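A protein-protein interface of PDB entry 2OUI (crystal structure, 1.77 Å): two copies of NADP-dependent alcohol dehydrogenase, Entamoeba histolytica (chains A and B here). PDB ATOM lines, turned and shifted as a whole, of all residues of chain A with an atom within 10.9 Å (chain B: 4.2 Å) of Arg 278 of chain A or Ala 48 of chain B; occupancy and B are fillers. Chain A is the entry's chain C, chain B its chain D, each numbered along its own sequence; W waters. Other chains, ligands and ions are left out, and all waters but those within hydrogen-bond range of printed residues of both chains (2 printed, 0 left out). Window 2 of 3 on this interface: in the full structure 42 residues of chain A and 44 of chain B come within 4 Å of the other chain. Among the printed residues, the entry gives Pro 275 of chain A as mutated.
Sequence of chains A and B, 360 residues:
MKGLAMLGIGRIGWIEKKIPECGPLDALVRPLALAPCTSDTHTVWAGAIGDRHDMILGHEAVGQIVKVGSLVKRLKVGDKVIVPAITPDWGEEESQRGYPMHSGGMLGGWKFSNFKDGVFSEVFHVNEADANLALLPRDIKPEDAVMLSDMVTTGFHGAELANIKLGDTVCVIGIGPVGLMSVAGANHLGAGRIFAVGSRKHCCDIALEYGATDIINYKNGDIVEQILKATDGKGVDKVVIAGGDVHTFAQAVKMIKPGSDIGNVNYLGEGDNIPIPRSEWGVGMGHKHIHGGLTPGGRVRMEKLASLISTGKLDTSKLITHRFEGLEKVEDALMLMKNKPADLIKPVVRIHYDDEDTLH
The backbone NH (N) of Ala 48 of chain B sits at hydrogen-bond distance from the backbone carbonyl oxygen (O) of His 42 of chain B (3.4 Å).
OH of Tyr 267 of chain B sits at hydrogen-bond distance from OG1 of Thr 43 of chain B (2.7 Å).
O of Arg 278 of chain A lies within hydrogen-bond range of N of Val 283 of chain A (2.9 Å).
The backbone carbonyl oxygen (O) of Leu 268 of chain B lies within hydrogen-bond range of the guanidinium group (NH1) of Arg 278 of chain A (3.1 Å).
O of Val 283 of chain A is in hydrogen-bond range of N of Leu 268 of chain B (2.9 Å).
NE of Arg 278 of chain A sits at hydrogen-bond distance from O of Gly 271 of chain B (2.7 Å).
The backbone NH of Arg 278 of chain A lies within hydrogen-bond range of the backbone carbonyl oxygen of Asp 272 of chain B, 2.9 Å away.
No position is printed for both chains.
Of the 11 pairs that touch across the chains among the printed residues, none has its exchanged pair printed and touching as well.
Water W1 bridges OG of Ser 279 of chain A (2.5 Å) and O of Ala 48 of chain B (3.0 Å).
Water W2 lies within hydrogen-bond range of O of Asp 272 of chain B (3.0 Å), N of Ser 279 of chain A (3.0 Å) and N of Arg 278 of chain A (3.4 Å).
Arg 278 of chain A touches just these residues of chain B: Ala 48, Leu 268, Gly 269, Glu 270, Gly 271 and Asp 272.
Printed residues of chain A within 4 Å of Ala 48 of chain B: Arg 278.
Thr 43 of chain B touches none of the printed residues of chain A.
No residue of chain A comes within 4 Å of Ala 46 of chain B.
No residue of chain A comes within 4 Å of Ile 49 of chain B.
No residue of chain A comes within 4 Å of Gly 50 of chain B.
Leu 268 of chain B touches three residues of chain A.
Gly 269 of chain B touches just one residue of chain A: Arg 278 (3.8 Å).
Printed residues of chain A within 4 Å of Tyr 267 of chain B: Val 283 and Met 285.
Printed residues of chain B within 4 Å of Pro 277 of chain A: Asp 272 (3.6 Å).
Val 253 of chain A touches none of the printed residues of chain B.
The nearest printed residue of chain B that does not touch Arg 278 of chain A is Tyr 267 of chain B (5.7 Å).
The nearest printed residue of chain A that does not touch Ala 48 of chain B is Val 283 of chain A (4.004 Å).
Of the 21 printed residues of chain A, 5 touch a printed residue of chain B.
Hydrophobic or aromatic side chains of chain A within 4 Å of the printed part of chain B: Val 283 and Met 285.
Of the 13 printed residues of chain B, 7 touch a printed residue of chain A.
Hydrophobic or aromatic side chains of chain B within 4 Å of the printed part of chain A: Tyr 267 and Leu 268.
Among the printed residues, no Asp or Glu carboxylate lies within 4 Å of a Lys or Arg side-chain nitrogen of the other chain.
Among the printed residues, merely in contact across the chains: Arg 278 of chain A with Glu 270 of chain B (3.4 Å), Met 285 of chain A with Tyr 267 of chain B (3.6 Å), Pro 277 of chain A with Asp 272 of chain B (3.6 Å), Val 283 of chain A with Tyr 267 of chain B (3.7 Å), Arg 278 of chain A with Gly 269 of chain B (3.8 Å), Arg 278 of chain A with Ala 48 of chain B (3.8 Å) and Gly 284 of chain A with Leu 268 of chain B (3.8 Å).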
ATOM      1  N   PHE A 249       4.967 -17.941 -29.655  1.00  0.00           N
ATOM      2  CA  PHE A 249       6.418 -18.119 -29.864  1.00  0.00           C
ATOM      3  C   PHE A 249       7.224 -17.357 -28.828  1.00  0.00           C
ATOM      4  O   PHE A 249       8.254 -17.850 -28.410  1.00  0.00           O
ATOM      5  CB  PHE A 249       6.821 -17.692 -31.266  1.00  0.00           C
ATOM      6  CG  PHE A 249       6.312 -18.628 -32.341  1.00  0.00           C
ATOM      7  CD1 PHE A 249       4.962 -18.600 -32.721  1.00  0.00           C
ATOM      8  CD2 PHE A 249       7.167 -19.540 -32.951  1.00  0.00           C
ATOM      9  CE1 PHE A 249       4.470 -19.474 -33.709  1.00  0.00           C
ATOM     10  CE2 PHE A 249       6.693 -20.411 -33.963  1.00  0.00           C
ATOM     11  CZ  PHE A 249       5.334 -20.363 -34.343  1.00  0.00           C
ATOM     12  N   ALA A 250       6.790 -16.153 -28.446  1.00  0.00           N
ATOM     13  CA  ALA A 250       7.525 -15.390 -27.415  1.00  0.00           C
ATOM     14  C   ALA A 250       7.496 -16.136 -26.085  1.00  0.00           C
ATOM     15  O   ALA A 250       8.488 -16.166 -25.360  1.00  0.00           O
ATOM     16  CB  ALA A 250       7.003 -13.997 -27.261  1.00  0.00           C
ATOM     17  N   GLN A 251       6.376 -16.797 -25.800  1.00  0.00           N
ATOM     18  CA  GLN A 251       6.269 -17.586 -24.579  1.00  0.00           C
ATOM     19  C   GLN A 251       7.236 -18.756 -24.616  1.00  0.00           C
ATOM     20  O   GLN A 251       7.897 -19.076 -23.610  1.00  0.00           O
ATOM     21  CB  GLN A 251       4.838 -18.084 -24.379  1.00  0.00           C
ATOM     22  CG  GLN A 251       3.843 -16.963 -24.120  1.00  0.00           C
ATOM     23  CD  GLN A 251       2.402 -17.469 -24.028  1.00  0.00           C
ATOM     24  OE1 GLN A 251       1.625 -17.009 -23.187  1.00  0.00           O
ATOM     25  NE2 GLN A 251       2.048 -18.422 -24.884  1.00  0.00           N
ATOM     26  N   VAL A 253      10.052 -18.932 -26.342  1.00  0.00           N
ATOM     27  CA  VAL A 253      11.421 -18.427 -26.210  1.00  0.00           C
ATOM     28  C   VAL A 253      11.740 -18.086 -24.753  1.00  0.00           C
ATOM     29  O   VAL A 253      12.849 -18.353 -24.294  1.00  0.00           O
ATOM     30  CB  VAL A 253      11.652 -17.201 -27.135  1.00  0.00           C
ATOM     31  CG1 VAL A 253      12.973 -16.485 -26.829  1.00  0.00           C
ATOM     32  CG2 VAL A 253      11.608 -17.662 -28.592  1.00  0.00           C
ATOM     33  N   LYS A 254      10.770 -17.529 -24.027  1.00  0.00           N
ATOM     34  CA  LYS A 254      10.994 -17.069 -22.671  1.00  0.00           C
ATOM     35  C   LYS A 254      11.114 -18.234 -21.690  1.00  0.00           C
ATOM     36  O   LYS A 254      11.703 -18.069 -20.625  1.00  0.00           O
ATOM     37  CB  LYS A 254       9.898 -16.123 -22.225  1.00  0.00           C
ATOM     38  CG  LYS A 254      10.018 -14.732 -22.930  1.00  0.00           C
ATOM     39  CD  LYS A 254       8.866 -13.818 -22.615  1.00  0.00           C
ATOM     40  CE  LYS A 254       8.911 -12.644 -23.565  1.00  0.00           C
ATOM     41  NZ  LYS A 254       7.892 -11.613 -23.225  1.00  0.00           N
ATOM     42  N   ILE A 274       5.229 -12.806 -36.574  1.00  0.00           N
ATOM     43  CA  ILE A 274       5.453 -13.582 -35.357  1.00  0.00           C
ATOM     44  C   ILE A 274       6.588 -12.863 -34.646  1.00  0.00           C
ATOM     45  O   ILE A 274       7.721 -12.861 -35.129  1.00  0.00           O
ATOM     46  CB  ILE A 274       5.884 -15.014 -35.714  1.00  0.00           C
ATOM     47  CG1 ILE A 274       4.789 -15.707 -36.539  1.00  0.00           C
ATOM     48  CG2 ILE A 274       6.256 -15.825 -34.474  1.00  0.00           C
ATOM     49  CD1 ILE A 274       5.359 -16.807 -37.450  1.00  0.00           C
ATOM     50  N   PRO A 275       6.285 -12.199 -33.521  1.00  0.00           N
ATOM     51  CA  PRO A 275       7.316 -11.472 -32.763  1.00  0.00           C
ATOM     52  C   PRO A 275       8.219 -12.416 -31.943  1.00  0.00           C
ATOM     53  O   PRO A 275       7.739 -13.142 -31.077  1.00  0.00           O
ATOM     54  CB  PRO A 275       6.497 -10.561 -31.836  1.00  0.00           C
ATOM     55  CG  PRO A 275       5.062 -10.702 -32.288  1.00  0.00           C
ATOM     56  CD  PRO A 275       4.943 -12.025 -32.937  1.00  0.00           C
ATOM     57  N   ILE A 276       9.519 -12.417 -32.243  1.00  0.00           N
ATOM     58  CA  ILE A 276      10.501 -13.153 -31.431  1.00  0.00           C
ATOM     59  C   ILE A 276      11.206 -12.136 -30.534  1.00  0.00           C
ATOM     60  O   ILE A 276      11.790 -11.164 -31.044  1.00  0.00           O
ATOM     61  CB  ILE A 276      11.518 -13.875 -32.331  1.00  0.00           C
ATOM     62  CG1 ILE A 276      10.795 -14.796 -33.332  1.00  0.00           C
ATOM     63  CG2 ILE A 276      12.560 -14.628 -31.481  1.00  0.00           C
ATOM     64  CD1 ILE A 276       9.786 -15.797 -32.679  1.00  0.00           C
ATOM     65  N   PRO A 277      11.129 -12.315 -29.193  1.00  0.00           N
ATOM     66  CA  PRO A 277      11.675 -11.278 -28.273  1.00  0.00           C
ATOM     67  C   PRO A 277      13.207 -11.225 -28.336  1.00  0.00           C
ATOM     68  O   PRO A 277      13.879 -12.258 -28.139  1.00  0.00           O
ATOM     69  CB  PRO A 277      11.185 -11.730 -26.885  1.00  0.00           C
ATOM     70  CG  PRO A 277      10.921 -13.188 -27.015  1.00  0.00           C
ATOM     71  CD  PRO A 277      10.548 -13.458 -28.455  1.00  0.00           C
ATOM     72  N   ARG A 278      13.753 -10.057 -28.669  1.00  0.00           N
ATOM     73  CA  ARG A 278      15.204  -9.944 -28.893  1.00  0.00           C
ATOM     74  C   ARG A 278      16.055 -10.378 -27.697  1.00  0.00           C
ATOM     75  O   ARG A 278      16.955 -11.212 -27.847  1.00  0.00           O
ATOM     76  CB  ARG A 278      15.590  -8.528 -29.355  1.00  0.00           C
ATOM     77  CG  ARG A 278      17.093  -8.322 -29.564  1.00  0.00           C
ATOM     78  CD  ARG A 278      17.442  -6.878 -29.975  1.00  0.00           C
ATOM     79  NE  ARG A 278      17.058  -5.895 -28.949  1.00  0.00           N
ATOM     80  CZ  ARG A 278      17.798  -5.561 -27.895  1.00  0.00           C
ATOM     81  NH1 ARG A 278      19.003  -6.076 -27.718  1.00  0.00           N
ATOM     82  NH2 ARG A 278      17.350  -4.661 -27.025  1.00  0.00           N
ATOM     83  N   SER A 279      15.773  -9.829 -26.516  1.00  0.00           N
ATOM     84  CA  SER A 279      16.589 -10.109 -25.336  1.00  0.00           C
ATOM     85  C   SER A 279      16.559 -11.587 -24.963  1.00  0.00           C
ATOM     86  O   SER A 279      17.615 -12.208 -24.770  1.00  0.00           O
ATOM     87  CB  SER A 279      16.172  -9.231 -24.150  1.00  0.00           C
ATOM     88  OG  SER A 279      16.717  -7.930 -24.285  1.00  0.00           O
ATOM     89  N   GLU A 280      15.360 -12.158 -24.881  1.00  0.00           N
ATOM     90  CA  GLU A 280      15.247 -13.565 -24.508  1.00  0.00           C
ATOM     91  C   GLU A 280      15.731 -14.526 -25.593  1.00  0.00           C
ATOM     92  O   GLU A 280      15.959 -15.692 -25.334  1.00  0.00           O
ATOM     93  CB  GLU A 280      13.805 -13.882 -24.100  1.00  0.00           C
ATOM     94  CG  GLU A 280      13.422 -13.166 -22.789  1.00  0.00           C
ATOM     95  CD  GLU A 280      12.766 -11.821 -22.969  1.00  0.00           C
ATOM     96  OE1 GLU A 280      12.155 -11.372 -21.971  1.00  0.00           O
ATOM     97  OE2 GLU A 280      12.861 -11.204 -24.068  1.00  0.00           O
ATOM     98  N   TRP A 281      15.873 -14.033 -26.817  1.00  0.00           N
ATOM     99  CA  TRP A 281      16.441 -14.860 -27.873  1.00  0.00           C
ATOM    100  C   TRP A 281      17.972 -14.713 -27.888  1.00  0.00           C
ATOM    101  O   TRP A 281      18.634 -15.050 -28.870  1.00  0.00           O
ATOM    102  CB  TRP A 281      15.811 -14.500 -29.236  1.00  0.00           C
ATOM    103  CG  TRP A 281      15.889 -15.642 -30.242  1.00  0.00           C
ATOM    104  CD1 TRP A 281      15.461 -16.923 -30.067  1.00  0.00           C
ATOM    105  CD2 TRP A 281      16.436 -15.573 -31.569  1.00  0.00           C
ATOM    106  NE1 TRP A 281      15.702 -17.671 -31.228  1.00  0.00           N
ATOM    107  CE2 TRP A 281      16.288 -16.846 -32.158  1.00  0.00           C
ATOM    108  CE3 TRP A 281      17.029 -14.534 -32.320  1.00  0.00           C
ATOM    109  CZ2 TRP A 281      16.761 -17.135 -33.448  1.00  0.00           C
ATOM    110  CZ3 TRP A 281      17.472 -14.809 -33.614  1.00  0.00           C
ATOM    111  CH2 TRP A 281      17.332 -16.102 -34.162  1.00  0.00           C
ATOM    112  N   GLY A 282      18.536 -14.165 -26.809  1.00  0.00           N
ATOM    113  CA  GLY A 282      19.995 -14.063 -26.664  1.00  0.00           C
ATOM    114  C   GLY A 282      20.552 -12.995 -27.577  1.00  0.00           C
ATOM    115  O   GLY A 282      21.669 -13.129 -28.079  1.00  0.00           O
ATOM    116  N   VAL A 283      19.774 -11.927 -27.768  1.00  0.00           N
ATOM    117  CA  VAL A 283      20.090 -10.834 -28.707  1.00  0.00           C
ATOM    118  C   VAL A 283      20.635 -11.350 -30.057  1.00  0.00           C
ATOM    119  O   VAL A 283      21.520 -10.741 -30.674  1.00  0.00           O
ATOM    120  CB  VAL A 283      20.949  -9.717 -28.058  1.00  0.00           C
ATOM    121  CG1 VAL A 283      20.179  -9.078 -26.898  1.00  0.00           C
ATOM    122  CG2 VAL A 283      22.352 -10.213 -27.596  1.00  0.00           C
ATOM    123  N   GLY A 284      20.048 -12.461 -30.504  1.00  0.00           N
ATOM    124  CA  GLY A 284      20.344 -13.092 -31.811  1.00  0.00           C
ATOM    125  C   GLY A 284      21.252 -14.312 -31.731  1.00  0.00           C
ATOM    126  O   GLY A 284      21.549 -14.922 -32.757  1.00  0.00           O
ATOM    127  N   MET A 285      21.663 -14.692 -30.518  1.00  0.00           N
ATOM    128  CA  MET A 285      22.785 -15.618 -30.394  1.00  0.00           C
ATOM    129  C   MET A 285      22.584 -16.724 -29.363  1.00  0.00           C
ATOM    130  O   MET A 285      23.549 -17.352 -28.985  1.00  0.00           O
ATOM    131  CB  MET A 285      24.064 -14.851 -30.042  1.00  0.00           C
ATOM    132  CG  MET A 285      24.445 -13.762 -31.088  1.00  0.00           C
ATOM    133  SD  MET A 285      25.918 -12.811 -30.694  1.00  0.00           S
ATOM    134  CE  MET A 285      25.294 -11.754 -29.391  1.00  0.00           C
ATOM    135  N   GLY A 286      21.354 -16.917 -28.895  1.00  0.00           N
ATOM    136  CA  GLY A 286      21.070 -17.903 -27.834  1.00  0.00           C
ATOM    137  C   GLY A 286      20.964 -19.367 -28.249  1.00  0.00           C
ATOM    138  O   GLY A 286      20.694 -20.233 -27.396  1.00  0.00           O
ATOM    139  N   HIS A 287      21.181 -19.664 -29.534  1.00  0.00           N
ATOM    140  CA  HIS A 287      20.941 -21.007 -30.099  1.00  0.00           C
ATOM    141  C   HIS A 287      19.577 -21.580 -29.643  1.00  0.00           C
ATOM    142  O   HIS A 287      19.463 -22.765 -29.304  1.00  0.00           O
ATOM    143  CB  HIS A 287      22.071 -22.005 -29.749  1.00  0.00           C
ATOM    144  CG  HIS A 287      23.365 -21.734 -30.448  1.00  0.00           C
ATOM    145  ND1 HIS A 287      24.339 -20.932 -29.899  1.00  0.00           N
ATOM    146  CD2 HIS A 287      23.844 -22.143 -31.653  1.00  0.00           C
ATOM    147  CE1 HIS A 287      25.380 -20.885 -30.716  1.00  0.00           C
ATOM    148  NE2 HIS A 287      25.111 -21.614 -31.786  1.00  0.00           N
ATOM    149  N   LYS A 288      18.542 -20.739 -29.648  1.00  0.00           N
ATOM    150  CA  LYS A 288      17.159 -21.182 -29.432  1.00  0.00           C
ATOM    151  C   LYS A 288      16.565 -21.361 -30.812  1.00  0.00           C
ATOM    152  O   LYS A 288      16.065 -20.399 -31.421  1.00  0.00           O
ATOM    153  CB  LYS A 288      16.380 -20.133 -28.605  1.00  0.00           C
ATOM    154  CG  LYS A 288      16.845 -20.100 -27.127  1.00  0.00           C
ATOM    155  CD  LYS A 288      16.166 -18.981 -26.326  1.00  0.00           C
ATOM    156  CE  LYS A 288      16.538 -19.082 -24.841  1.00  0.00           C
ATOM    157  NZ  LYS A 288      15.709 -18.148 -24.037  1.00  0.00           N
ATOM    158  N   ILE A 290      14.406 -22.148 -34.005  1.00  0.00           N
ATOM    159  CA  ILE A 290      12.963 -22.036 -34.195  1.00  0.00           C
ATOM    160  C   ILE A 290      12.580 -22.791 -35.482  1.00  0.00           C
ATOM    161  O   ILE A 290      13.081 -22.463 -36.569  1.00  0.00           O
ATOM    162  CB  ILE A 290      12.530 -20.576 -34.298  1.00  0.00           C
ATOM    163  CG1 ILE A 290      12.854 -19.813 -32.990  1.00  0.00           C
ATOM    164  CG2 ILE A 290      11.020 -20.481 -34.566  1.00  0.00           C
ATOM    165  CD1 ILE A 290      12.809 -18.298 -33.157  1.00  0.00           C
ATOM    166  N   HIS B  42      28.036  -1.850 -29.711  1.00  0.00           N
ATOM    167  CA  HIS B  42      26.638  -2.086 -29.268  1.00  0.00           C
ATOM    168  C   HIS B  42      26.595  -2.082 -27.745  1.00  0.00           C
ATOM    169  O   HIS B  42      25.760  -1.411 -27.127  1.00  0.00           O
ATOM    170  CB  HIS B  42      26.056  -3.419 -29.765  1.00  0.00           C
ATOM    171  CG  HIS B  42      26.096  -3.620 -31.251  1.00  0.00           C
ATOM    172  ND1 HIS B  42      25.940  -2.589 -32.156  1.00  0.00           N
ATOM    173  CD2 HIS B  42      26.224  -4.751 -31.988  1.00  0.00           C
ATOM    174  CE1 HIS B  42      26.006  -3.075 -33.387  1.00  0.00           C
ATOM    175  NE2 HIS B  42      26.173  -4.387 -33.311  1.00  0.00           N
ATOM    176  N   THR B  43      27.510  -2.840 -27.142  1.00  0.00           N
ATOM    177  CA  THR B  43      27.587  -2.936 -25.689  1.00  0.00           C
ATOM    178  C   THR B  43      27.767  -1.591 -24.993  1.00  0.00           C
ATOM    179  O   THR B  43      27.007  -1.260 -24.062  1.00  0.00           O
ATOM    180  CB  THR B  43      28.650  -3.957 -25.280  1.00  0.00           C
ATOM    181  OG1 THR B  43      28.288  -5.216 -25.862  1.00  0.00           O
ATOM    182  CG2 THR B  43      28.740  -4.089 -23.749  1.00  0.00           C
ATOM    183  N   ALA B  46      25.006   1.440 -27.177  1.00  0.00           N
ATOM    184  CA  ALA B  46      23.580   1.098 -27.224  1.00  0.00           C
ATOM    185  C   ALA B  46      23.114   0.443 -25.919  1.00  0.00           C
ATOM    186  O   ALA B  46      21.912   0.303 -25.688  1.00  0.00           O
ATOM    187  CB  ALA B  46      23.281   0.174 -28.420  1.00  0.00           C
ATOM    188  N   GLY B  47      24.057   0.037 -25.073  1.00  0.00           N
ATOM    189  CA  GLY B  47      23.716  -0.654 -23.832  1.00  0.00           C
ATOM    190  C   GLY B  47      22.956  -1.947 -24.096  1.00  0.00           C
ATOM    191  O   GLY B  47      22.083  -2.320 -23.318  1.00  0.00           O
ATOM    192  N   ALA B  48      23.333  -2.648 -25.166  1.00  0.00           N
ATOM    193  CA  ALA B  48      22.554  -3.777 -25.705  1.00  0.00           C
ATOM    194  C   ALA B  48      22.502  -5.013 -24.810  1.00  0.00           C
ATOM    195  O   ALA B  48      21.619  -5.870 -24.982  1.00  0.00           O
ATOM    196  CB  ALA B  48      23.068  -4.158 -27.106  1.00  0.00           C
ATOM    197  N   ILE B  49      23.465  -5.129 -23.897  1.00  0.00           N
ATOM    198  CA  ILE B  49      23.503  -6.267 -22.957  1.00  0.00           C
ATOM    199  C   ILE B  49      23.562  -5.800 -21.501  1.00  0.00           C
ATOM    200  O   ILE B  49      24.049  -6.531 -20.617  1.00  0.00           O
ATOM    201  CB  ILE B  49      24.629  -7.293 -23.271  1.00  0.00           C
ATOM    202  CG1 ILE B  49      25.999  -6.612 -23.466  1.00  0.00           C
ATOM    203  CG2 ILE B  49      24.229  -8.181 -24.477  1.00  0.00           C
ATOM    204  CD1 ILE B  49      27.167  -7.568 -23.434  1.00  0.00           C
ATOM    205  N   GLY B  50      23.063  -4.580 -21.282  1.00  0.00           N
ATOM    206  CA  GLY B  50      22.950  -3.977 -19.951  1.00  0.00           C
ATOM    207  C   GLY B  50      24.092  -3.052 -19.592  1.00  0.00           C
ATOM    208  O   GLY B  50      25.105  -3.033 -20.284  1.00  0.00           O
ATOM    209  N   TYR B 267      24.797  -9.812 -33.690  1.00  0.00           N
ATOM    210  CA  TYR B 267      24.423  -9.305 -32.368  1.00  0.00           C
ATOM    211  C   TYR B 267      23.463  -8.124 -32.550  1.00  0.00           C
ATOM    212  O   TYR B 267      23.837  -7.044 -33.061  1.00  0.00           O
ATOM    213  CB  TYR B 267      25.725  -8.955 -31.635  1.00  0.00           C
ATOM    214  CG  TYR B 267      25.678  -8.202 -30.314  1.00  0.00           C
ATOM    215  CD1 TYR B 267      26.863  -7.704 -29.791  1.00  0.00           C
ATOM    216  CD2 TYR B 267      24.494  -7.958 -29.614  1.00  0.00           C
ATOM    217  CE1 TYR B 267      26.894  -7.002 -28.609  1.00  0.00           C
ATOM    218  CE2 TYR B 267      24.513  -7.230 -28.404  1.00  0.00           C
ATOM    219  CZ  TYR B 267      25.729  -6.763 -27.922  1.00  0.00           C
ATOM    220  OH  TYR B 267      25.834  -6.025 -26.758  1.00  0.00           O
ATOM    221  N   LEU B 268      22.216  -8.348 -32.140  1.00  0.00           N
ATOM    222  CA  LEU B 268      21.113  -7.427 -32.405  1.00  0.00           C
ATOM    223  C   LEU B 268      21.076  -6.462 -31.250  1.00  0.00           C
ATOM    224  O   LEU B 268      20.811  -6.871 -30.107  1.00  0.00           O
ATOM    225  CB  LEU B 268      19.790  -8.197 -32.493  1.00  0.00           C
ATOM    226  CG  LEU B 268      19.745  -9.274 -33.577  1.00  0.00           C
ATOM    227  CD1 LEU B 268      18.508 -10.166 -33.422  1.00  0.00           C
ATOM    228  CD2 LEU B 268      19.748  -8.615 -34.937  1.00  0.00           C
ATOM    229  N   GLY B 269      21.342  -5.189 -31.545  1.00  0.00           N
ATOM    230  CA  GLY B 269      21.556  -4.170 -30.512  1.00  0.00           C
ATOM    231  C   GLY B 269      20.345  -3.397 -30.036  1.00  0.00           C
ATOM    232  O   GLY B 269      20.406  -2.760 -28.984  1.00  0.00           O
ATOM    233  N   GLU B 270      19.252  -3.428 -30.799  1.00  0.00           N
ATOM    234  CA  GLU B 270      18.031  -2.706 -30.436  1.00  0.00           C
ATOM    235  C   GLU B 270      16.789  -3.312 -31.085  1.00  0.00           C
ATOM    236  O   GLU B 270      16.901  -4.095 -32.034  1.00  0.00           O
ATOM    237  CB  GLU B 270      18.148  -1.229 -30.808  1.00  0.00           C
ATOM    238  CG  GLU B 270      18.283  -0.970 -32.278  1.00  0.00           C
ATOM    239  CD  GLU B 270      18.533   0.509 -32.577  1.00  0.00           C
ATOM    240  OE1 GLU B 270      19.371   0.803 -33.461  1.00  0.00           O
ATOM    241  OE2 GLU B 270      17.897   1.370 -31.921  1.00  0.00           O
ATOM    242  N   GLY B 271      15.627  -2.973 -30.526  1.00  0.00           N
ATOM    243  CA  GLY B 271      14.330  -3.434 -31.013  1.00  0.00           C
ATOM    244  C   GLY B 271      13.781  -4.446 -30.039  1.00  0.00           C
ATOM    245  O   GLY B 271      14.524  -5.323 -29.588  1.00  0.00           O
ATOM    246  N   ASP B 272      12.500  -4.336 -29.691  1.00  0.00           N
ATOM    247  CA  ASP B 272      11.938  -5.286 -28.724  1.00  0.00           C
ATOM    248  C   ASP B 272      11.810  -6.675 -29.327  1.00  0.00           C
ATOM    249  O   ASP B 272      12.098  -7.674 -28.657  1.00  0.00           O
ATOM    250  CB  ASP B 272      10.567  -4.857 -28.247  1.00  0.00           C
ATOM    251  CG  ASP B 272      10.609  -3.627 -27.372  1.00  0.00           C
ATOM    252  OD1 ASP B 272      11.715  -3.211 -26.939  1.00  0.00           O
ATOM    253  OD2 ASP B 272       9.513  -3.091 -27.114  1.00  0.00           O
HETATM  254  O   HOH W   1      19.148  -7.277 -23.990  1.00  0.00           O
HETATM  255  O   HOH W   2      13.598  -7.826 -26.103  1.00  0.00           O
